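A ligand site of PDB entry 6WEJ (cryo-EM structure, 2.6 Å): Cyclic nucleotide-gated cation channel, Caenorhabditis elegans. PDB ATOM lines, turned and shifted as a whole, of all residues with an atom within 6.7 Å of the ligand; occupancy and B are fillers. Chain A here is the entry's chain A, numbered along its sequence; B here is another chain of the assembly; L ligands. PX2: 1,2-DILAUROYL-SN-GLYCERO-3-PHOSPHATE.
The side-chain sulfur (SD) of Met 417 of chain B lies close to an oxygen (O8) of the ligand, 3.7 Å away. Residues that only touch the ligand: Tyr 315, Ile 319, Ile 402, Thr 405 and Met 413 of chain B. Hydrophobic or aromatic side chains within 4 Å of the ligand: Tyr 315, Ile 319, Ile 402, Met 413 of chain B and Met 417 of chain B.
O3 of the ligand is in salt-bridge range of NH1 of Arg 291 (3.1 Å). An oxygen (O7) of the ligand sits close to the side-chain amide oxygen of Asn 409, at 3.5 Å.
The side-chain hydroxyl (OG1) of Thr 405 lies within hydrogen-bond range of the backbone carbonyl oxygen (O) of Leu 401. The backbone carbonyl oxygen of Thr 405 sits close to the side-chain amide oxygen of Asn 409 (3.0 Å).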
ATOM      1  N   ARG A 291      33.467  22.588 -33.402  1.00  0.00           N
ATOM      2  CA  ARG A 291      33.784  22.837 -31.994  1.00  0.00           C
ATOM      3  C   ARG A 291      35.223  23.289 -31.828  1.00  0.00           C
ATOM      4  O   ARG A 291      35.512  24.186 -31.031  1.00  0.00           O
ATOM      5  CB  ARG A 291      33.526  21.575 -31.168  1.00  0.00           C
ATOM      6  CG  ARG A 291      32.077  21.140 -31.155  1.00  0.00           C
ATOM      7  CD  ARG A 291      31.282  21.867 -30.101  1.00  0.00           C
ATOM      8  NE  ARG A 291      31.462  21.282 -28.773  1.00  0.00           N
ATOM      9  CZ  ARG A 291      30.821  21.692 -27.683  1.00  0.00           C
ATOM     10  NH1 ARG A 291      29.963  22.699 -27.759  1.00  0.00           N
ATOM     11  NH2 ARG A 291      31.038  21.095 -26.518  1.00  0.00           N
ATOM     12  N   LEU A 294      35.446  26.906 -32.858  1.00  0.00           N
ATOM     13  CA  LEU A 294      34.840  27.807 -31.891  1.00  0.00           C
ATOM     14  C   LEU A 294      35.721  27.971 -30.654  1.00  0.00           C
ATOM     15  O   LEU A 294      35.870  29.084 -30.131  1.00  0.00           O
ATOM     16  CB  LEU A 294      33.450  27.324 -31.501  1.00  0.00           C
ATOM     17  CG  LEU A 294      32.432  27.429 -32.624  1.00  0.00           C
ATOM     18  CD1 LEU A 294      31.062  26.981 -32.152  1.00  0.00           C
ATOM     19  CD2 LEU A 294      32.383  28.840 -33.160  1.00  0.00           C
ATOM     20  N   GLU A 298      37.645  31.270 -29.354  1.00  0.00           N
ATOM     21  CA  GLU A 298      37.464  31.805 -28.009  1.00  0.00           C
ATOM     22  C   GLU A 298      38.809  32.112 -27.357  1.00  0.00           C
ATOM     23  O   GLU A 298      38.943  33.133 -26.681  1.00  0.00           O
ATOM     24  CB  GLU A 298      36.664  30.834 -27.161  1.00  0.00           C
ATOM     25  CG  GLU A 298      36.487  31.277 -25.724  1.00  0.00           C
ATOM     26  CD  GLU A 298      35.600  30.337 -24.940  1.00  0.00           C
ATOM     27  OE1 GLU A 298      34.414  30.669 -24.737  1.00  0.00           O
ATOM     28  OE2 GLU A 298      36.070  29.259 -24.536  1.00  0.00           O
ATOM     29  N   ARG A 308      31.587  34.046 -25.807  1.00  0.00           N
ATOM     30  CA  ARG A 308      30.809  32.908 -25.323  1.00  0.00           C
ATOM     31  C   ARG A 308      29.318  33.186 -25.407  1.00  0.00           C
ATOM     32  O   ARG A 308      28.542  32.369 -25.919  1.00  0.00           O
ATOM     33  CB  ARG A 308      31.241  32.571 -23.892  1.00  0.00           C
ATOM     34  CG  ARG A 308      30.566  31.359 -23.277  1.00  0.00           C
ATOM     35  CD  ARG A 308      31.516  30.654 -22.312  1.00  0.00           C
ATOM     36  NE  ARG A 308      32.313  31.596 -21.533  1.00  0.00           N
ATOM     37  CZ  ARG A 308      33.218  31.227 -20.631  1.00  0.00           C
ATOM     38  NH1 ARG A 308      33.901  32.154 -19.969  1.00  0.00           N
ATOM     39  NH2 ARG A 308      33.452  29.950 -20.388  1.00  0.00           N
ATOM     40  N   VAL A 311      28.252  33.159 -29.192  1.00  0.00           N
ATOM     41  CA  VAL A 311      28.035  31.855 -29.802  1.00  0.00           C
ATOM     42  C   VAL A 311      26.818  31.184 -29.193  1.00  0.00           C
ATOM     43  O   VAL A 311      26.142  30.397 -29.866  1.00  0.00           O
ATOM     44  CB  VAL A 311      29.288  30.964 -29.703  1.00  0.00           C
ATOM     45  CG1 VAL A 311      30.470  31.648 -30.351  1.00  0.00           C
ATOM     46  CG2 VAL A 311      29.594  30.609 -28.278  1.00  0.00           C
ATOM     47  N   VAL A 312      26.488  31.499 -27.944  1.00  0.00           N
ATOM     48  CA  VAL A 312      25.248  30.939 -27.385  1.00  0.00           C
ATOM     49  C   VAL A 312      24.032  31.535 -28.071  1.00  0.00           C
ATOM     50  O   VAL A 312      23.048  30.831 -28.343  1.00  0.00           O
ATOM     51  CB  VAL A 312      25.212  31.142 -25.859  1.00  0.00           C
ATOM     52  CG1 VAL A 312      23.812  30.878 -25.334  1.00  0.00           C
ATOM     53  CG2 VAL A 312      26.186  30.198 -25.196  1.00  0.00           C
ATOM     54  N   TYR A 315      23.674  29.842 -31.359  1.00  0.00           N
ATOM     55  CA  TYR A 315      23.018  28.569 -31.110  1.00  0.00           C
ATOM     56  C   TYR A 315      21.509  28.745 -30.974  1.00  0.00           C
ATOM     57  O   TYR A 315      20.738  27.956 -31.510  1.00  0.00           O
ATOM     58  CB  TYR A 315      23.576  27.919 -29.851  1.00  0.00           C
ATOM     59  CG  TYR A 315      24.940  27.308 -30.005  1.00  0.00           C
ATOM     60  CD1 TYR A 315      25.416  26.938 -31.248  1.00  0.00           C
ATOM     61  CD2 TYR A 315      25.747  27.087 -28.909  1.00  0.00           C
ATOM     62  CE1 TYR A 315      26.655  26.376 -31.387  1.00  0.00           C
ATOM     63  CE2 TYR A 315      26.995  26.533 -29.040  1.00  0.00           C
ATOM     64  CZ  TYR A 315      27.440  26.174 -30.285  1.00  0.00           C
ATOM     65  OH  TYR A 315      28.688  25.610 -30.420  1.00  0.00           O
ATOM     66  N   ILE A 316      21.091  29.773 -30.241  1.00  0.00           N
ATOM     67  CA  ILE A 316      19.664  29.972 -30.014  1.00  0.00           C
ATOM     68  C   ILE A 316      18.965  30.361 -31.307  1.00  0.00           C
ATOM     69  O   ILE A 316      17.843  29.938 -31.569  1.00  0.00           O
ATOM     70  CB  ILE A 316      19.431  31.025 -28.905  1.00  0.00           C
ATOM     71  CG1 ILE A 316      20.062  30.557 -27.593  1.00  0.00           C
ATOM     72  CG2 ILE A 316      17.957  31.264 -28.705  1.00  0.00           C
ATOM     73  CD1 ILE A 316      19.671  29.164 -27.172  1.00  0.00           C
ATOM     74  N   ILE A 319      18.523  27.256 -33.274  1.00  0.00           N
ATOM     75  CA  ILE A 319      17.440  26.450 -32.704  1.00  0.00           C
ATOM     76  C   ILE A 319      16.079  27.048 -33.066  1.00  0.00           C
ATOM     77  O   ILE A 319      15.135  26.321 -33.335  1.00  0.00           O
ATOM     78  CB  ILE A 319      17.622  26.327 -31.181  1.00  0.00           C
ATOM     79  CG1 ILE A 319      18.869  25.515 -30.869  1.00  0.00           C
ATOM     80  CG2 ILE A 319      16.427  25.659 -30.548  1.00  0.00           C
ATOM     81  CD1 ILE A 319      19.192  25.432 -29.408  1.00  0.00           C
ATOM     82  N   MET A 397       8.126  23.825 -22.841  1.00  0.00           N
ATOM     83  CA  MET A 397       9.088  23.360 -21.840  1.00  0.00           C
ATOM     84  C   MET A 397      10.517  23.505 -22.351  1.00  0.00           C
ATOM     85  O   MET A 397      11.409  23.965 -21.611  1.00  0.00           O
ATOM     86  CB  MET A 397       8.761  21.922 -21.445  1.00  0.00           C
ATOM     87  CG  MET A 397       7.374  21.797 -20.832  1.00  0.00           C
ATOM     88  SD  MET A 397       7.003  20.252 -19.969  1.00  0.00           S
ATOM     89  CE  MET A 397       6.888  19.101 -21.321  1.00  0.00           C
ATOM     90  N   CYS A 398      10.757  23.153 -23.616  1.00  0.00           N
ATOM     91  CA  CYS A 398      12.065  23.418 -24.206  1.00  0.00           C
ATOM     92  C   CYS A 398      12.390  24.907 -24.205  1.00  0.00           C
ATOM     93  O   CYS A 398      13.541  25.296 -24.032  1.00  0.00           O
ATOM     94  CB  CYS A 398      12.114  22.868 -25.631  1.00  0.00           C
ATOM     95  SG  CYS A 398      11.914  21.090 -25.749  1.00  0.00           S
ATOM     96  N   GLY A 399      11.385  25.755 -24.402  1.00  0.00           N
ATOM     97  CA  GLY A 399      11.624  27.186 -24.385  1.00  0.00           C
ATOM     98  C   GLY A 399      11.933  27.716 -23.000  1.00  0.00           C
ATOM     99  O   GLY A 399      12.714  28.651 -22.854  1.00  0.00           O
ATOM    100  N   LEU A 401      13.588  25.964 -20.817  1.00  0.00           N
ATOM    101  CA  LEU A 401      14.990  25.592 -20.635  1.00  0.00           C
ATOM    102  C   LEU A 401      15.926  26.485 -21.441  1.00  0.00           C
ATOM    103  O   LEU A 401      17.022  26.834 -20.978  1.00  0.00           O
ATOM    104  CB  LEU A 401      15.210  24.131 -20.997  1.00  0.00           C
ATOM    105  CG  LEU A 401      14.589  23.138 -20.019  1.00  0.00           C
ATOM    106  CD1 LEU A 401      14.844  21.719 -20.479  1.00  0.00           C
ATOM    107  CD2 LEU A 401      15.152  23.352 -18.637  1.00  0.00           C
ATOM    108  N   ILE A 402      15.515  26.896 -22.645  1.00  0.00           N
ATOM    109  CA  ILE A 402      16.343  27.766 -23.473  1.00  0.00           C
ATOM    110  C   ILE A 402      16.459  29.153 -22.858  1.00  0.00           C
ATOM    111  O   ILE A 402      17.543  29.759 -22.835  1.00  0.00           O
ATOM    112  CB  ILE A 402      15.759  27.838 -24.895  1.00  0.00           C
ATOM    113  CG1 ILE A 402      16.112  26.572 -25.669  1.00  0.00           C
ATOM    114  CG2 ILE A 402      16.246  29.067 -25.625  1.00  0.00           C
ATOM    115  CD1 ILE A 402      15.436  26.486 -26.991  1.00  0.00           C
ATOM    116  N   PHE A 403      15.347  29.692 -22.355  1.00  0.00           N
ATOM    117  CA  PHE A 403      15.377  30.970 -21.657  1.00  0.00           C
ATOM    118  C   PHE A 403      16.263  30.902 -20.419  1.00  0.00           C
ATOM    119  O   PHE A 403      17.026  31.840 -20.151  1.00  0.00           O
ATOM    120  CB  PHE A 403      13.949  31.377 -21.293  1.00  0.00           C
ATOM    121  CG  PHE A 403      13.841  32.724 -20.677  1.00  0.00           C
ATOM    122  CD1 PHE A 403      13.759  33.859 -21.462  1.00  0.00           C
ATOM    123  CD2 PHE A 403      13.795  32.872 -19.306  1.00  0.00           C
ATOM    124  CE1 PHE A 403      13.646  35.096 -20.895  1.00  0.00           C
ATOM    125  CE2 PHE A 403      13.681  34.118 -18.736  1.00  0.00           C
ATOM    126  CZ  PHE A 403      13.609  35.232 -19.523  1.00  0.00           C
ATOM    127  N   THR A 405      18.778  28.961 -20.051  1.00  0.00           N
ATOM    128  CA  THR A 405      20.162  28.894 -20.524  1.00  0.00           C
ATOM    129  C   THR A 405      20.689  30.264 -20.910  1.00  0.00           C
ATOM    130  O   THR A 405      21.835  30.615 -20.585  1.00  0.00           O
ATOM    131  CB  THR A 405      20.251  27.943 -21.719  1.00  0.00           C
ATOM    132  OG1 THR A 405      19.986  26.606 -21.279  1.00  0.00           O
ATOM    133  CG2 THR A 405      21.619  27.997 -22.341  1.00  0.00           C
ATOM    134  N   ASN A 409      23.795  32.080 -18.975  1.00  0.00           N
ATOM    135  CA  ASN A 409      25.035  32.473 -19.634  1.00  0.00           C
ATOM    136  C   ASN A 409      25.293  33.965 -19.479  1.00  0.00           C
ATOM    137  O   ASN A 409      26.423  34.377 -19.215  1.00  0.00           O
ATOM    138  CB  ASN A 409      24.996  32.098 -21.114  1.00  0.00           C
ATOM    139  CG  ASN A 409      25.418  30.669 -21.351  1.00  0.00           C
ATOM    140  OD1 ASN A 409      24.602  29.761 -21.353  1.00  0.00           O
ATOM    141  ND2 ASN A 409      26.714  30.461 -21.548  1.00  0.00           N
ATOM    142  N   VAL B 309      20.161  18.714 -13.133  1.00  0.00           N
ATOM    143  CA  VAL B 309      19.122  19.477 -13.820  1.00  0.00           C
ATOM    144  C   VAL B 309      18.028  18.567 -14.364  1.00  0.00           C
ATOM    145  O   VAL B 309      16.844  18.936 -14.375  1.00  0.00           O
ATOM    146  CB  VAL B 309      19.745  20.355 -14.929  1.00  0.00           C
ATOM    147  CG1 VAL B 309      18.689  21.207 -15.598  1.00  0.00           C
ATOM    148  CG2 VAL B 309      20.819  21.248 -14.330  1.00  0.00           C
ATOM    149  N   VAL B 410      19.658  25.769 -13.570  1.00  0.00           N
ATOM    150  CA  VAL B 410      20.376  25.848 -14.843  1.00  0.00           C
ATOM    151  C   VAL B 410      21.531  26.828 -14.744  1.00  0.00           C
ATOM    152  O   VAL B 410      22.609  26.583 -15.280  1.00  0.00           O
ATOM    153  CB  VAL B 410      19.407  26.208 -15.976  1.00  0.00           C
ATOM    154  CG1 VAL B 410      20.168  26.437 -17.261  1.00  0.00           C
ATOM    155  CG2 VAL B 410      18.397  25.103 -16.176  1.00  0.00           C
ATOM    156  N   MET B 413      24.333  25.134 -12.866  1.00  0.00           N
ATOM    157  CA  MET B 413      25.030  24.191 -13.735  1.00  0.00           C
ATOM    158  C   MET B 413      25.946  24.919 -14.713  1.00  0.00           C
ATOM    159  O   MET B 413      27.082  24.491 -14.939  1.00  0.00           O
ATOM    160  CB  MET B 413      24.029  23.342 -14.506  1.00  0.00           C
ATOM    161  CG  MET B 413      24.672  22.436 -15.525  1.00  0.00           C
ATOM    162  SD  MET B 413      23.560  21.781 -16.764  1.00  0.00           S
ATOM    163  CE  MET B 413      23.024  23.292 -17.534  1.00  0.00           C
ATOM    164  N   ILE B 414      25.468  26.013 -15.296  1.00  0.00           N
ATOM    165  CA  ILE B 414      26.286  26.775 -16.247  1.00  0.00           C
ATOM    166  C   ILE B 414      27.495  27.381 -15.542  1.00  0.00           C
ATOM    167  O   ILE B 414      28.584  27.440 -16.107  1.00  0.00           O
ATOM    168  CB  ILE B 414      25.435  27.851 -16.930  1.00  0.00           C
ATOM    169  CG1 ILE B 414      24.397  27.207 -17.847  1.00  0.00           C
ATOM    170  CG2 ILE B 414      26.304  28.803 -17.720  1.00  0.00           C
ATOM    171  CD1 ILE B 414      23.443  28.188 -18.428  1.00  0.00           C
ATOM    172  N   MET B 417      30.141  24.440 -14.747  1.00  0.00           N
ATOM    173  CA  MET B 417      30.829  23.835 -15.884  1.00  0.00           C
ATOM    174  C   MET B 417      31.742  24.801 -16.621  1.00  0.00           C
ATOM    175  O   MET B 417      32.457  24.364 -17.533  1.00  0.00           O
ATOM    176  CB  MET B 417      29.825  23.229 -16.854  1.00  0.00           C
ATOM    177  CG  MET B 417      28.878  24.235 -17.483  1.00  0.00           C
ATOM    178  SD  MET B 417      27.826  23.464 -18.724  1.00  0.00           S
ATOM    179  CE  MET B 417      27.587  21.862 -17.983  1.00  0.00           C
ATOM    180  N   SER B 418      31.752  26.071 -16.260  1.00  0.00           N
ATOM    181  CA  SER B 418      32.651  27.045 -16.858  1.00  0.00           C
ATOM    182  C   SER B 418      33.532  27.720 -15.805  1.00  0.00           C
ATOM    183  O   SER B 418      33.978  28.852 -16.002  1.00  0.00           O
ATOM    184  CB  SER B 418      31.857  28.098 -17.635  1.00  0.00           C
ATOM    185  OG  SER B 418      31.113  28.925 -16.758  1.00  0.00           O
HETATM  186  O1  PX2 L   1      29.552  23.651 -24.178  1.00  0.00           O
HETATM  187  O2  PX2 L   1      30.247  25.966 -23.714  1.00  0.00           O
HETATM  188  P1  PX2 L   1      29.388  25.098 -24.589  1.00  0.00           P
HETATM  189  O3  PX2 L   1      29.799  25.265 -26.034  1.00  0.00           O
HETATM  190  O4  PX2 L   1      27.806  25.538 -24.423  1.00  0.00           O
HETATM  191  C1  PX2 L   1      27.410  26.130 -23.218  1.00  0.00           C
HETATM  192  C2  PX2 L   1      25.919  26.484 -23.277  1.00  0.00           C
HETATM  193  C3  PX2 L   1      25.202  25.584 -24.284  1.00  0.00           C
HETATM  194  O5  PX2 L   1      24.635  26.367 -25.304  1.00  0.00           O
HETATM  195  C4  PX2 L   1      23.590  25.741 -25.981  1.00  0.00           C
HETATM  196  O6  PX2 L   1      23.819  24.799 -26.651  1.00  0.00           O
HETATM  197  C5  PX2 L   1      22.162  26.262 -25.844  1.00  0.00           C
HETATM  198  C6  PX2 L   1      21.197  25.106 -26.082  1.00  0.00           C
HETATM  199  C7  PX2 L   1      19.968  25.250 -25.198  1.00  0.00           C
HETATM  200  C8  PX2 L   1      19.608  23.895 -24.603  1.00  0.00           C
HETATM  201  C9  PX2 L   1      18.262  23.970 -23.891  1.00  0.00           C
HETATM  202  C10 PX2 L   1      17.278  23.013 -24.555  1.00  0.00           C
HETATM  203  O7  PX2 L   1      25.349  26.404 -22.004  1.00  0.00           O
HETATM  204  C16 PX2 L   1      24.889  25.147 -21.578  1.00  0.00           C
HETATM  205  O8  PX2 L   1      25.611  24.208 -21.548  1.00  0.00           O
HETATM  206  C17 PX2 L   1      23.448  24.980 -21.094  1.00  0.00           C
HETATM  207  C18 PX2 L   1      22.724  23.958 -21.952  1.00  0.00           C
HETATM  208  C19 PX2 L   1      21.989  22.965 -21.038  1.00  0.00           C
HETATM  209  C20 PX2 L   1      20.544  23.411 -20.827  1.00  0.00           C
HETATM  210  C21 PX2 L   1      19.774  22.308 -20.124  1.00  0.00           C
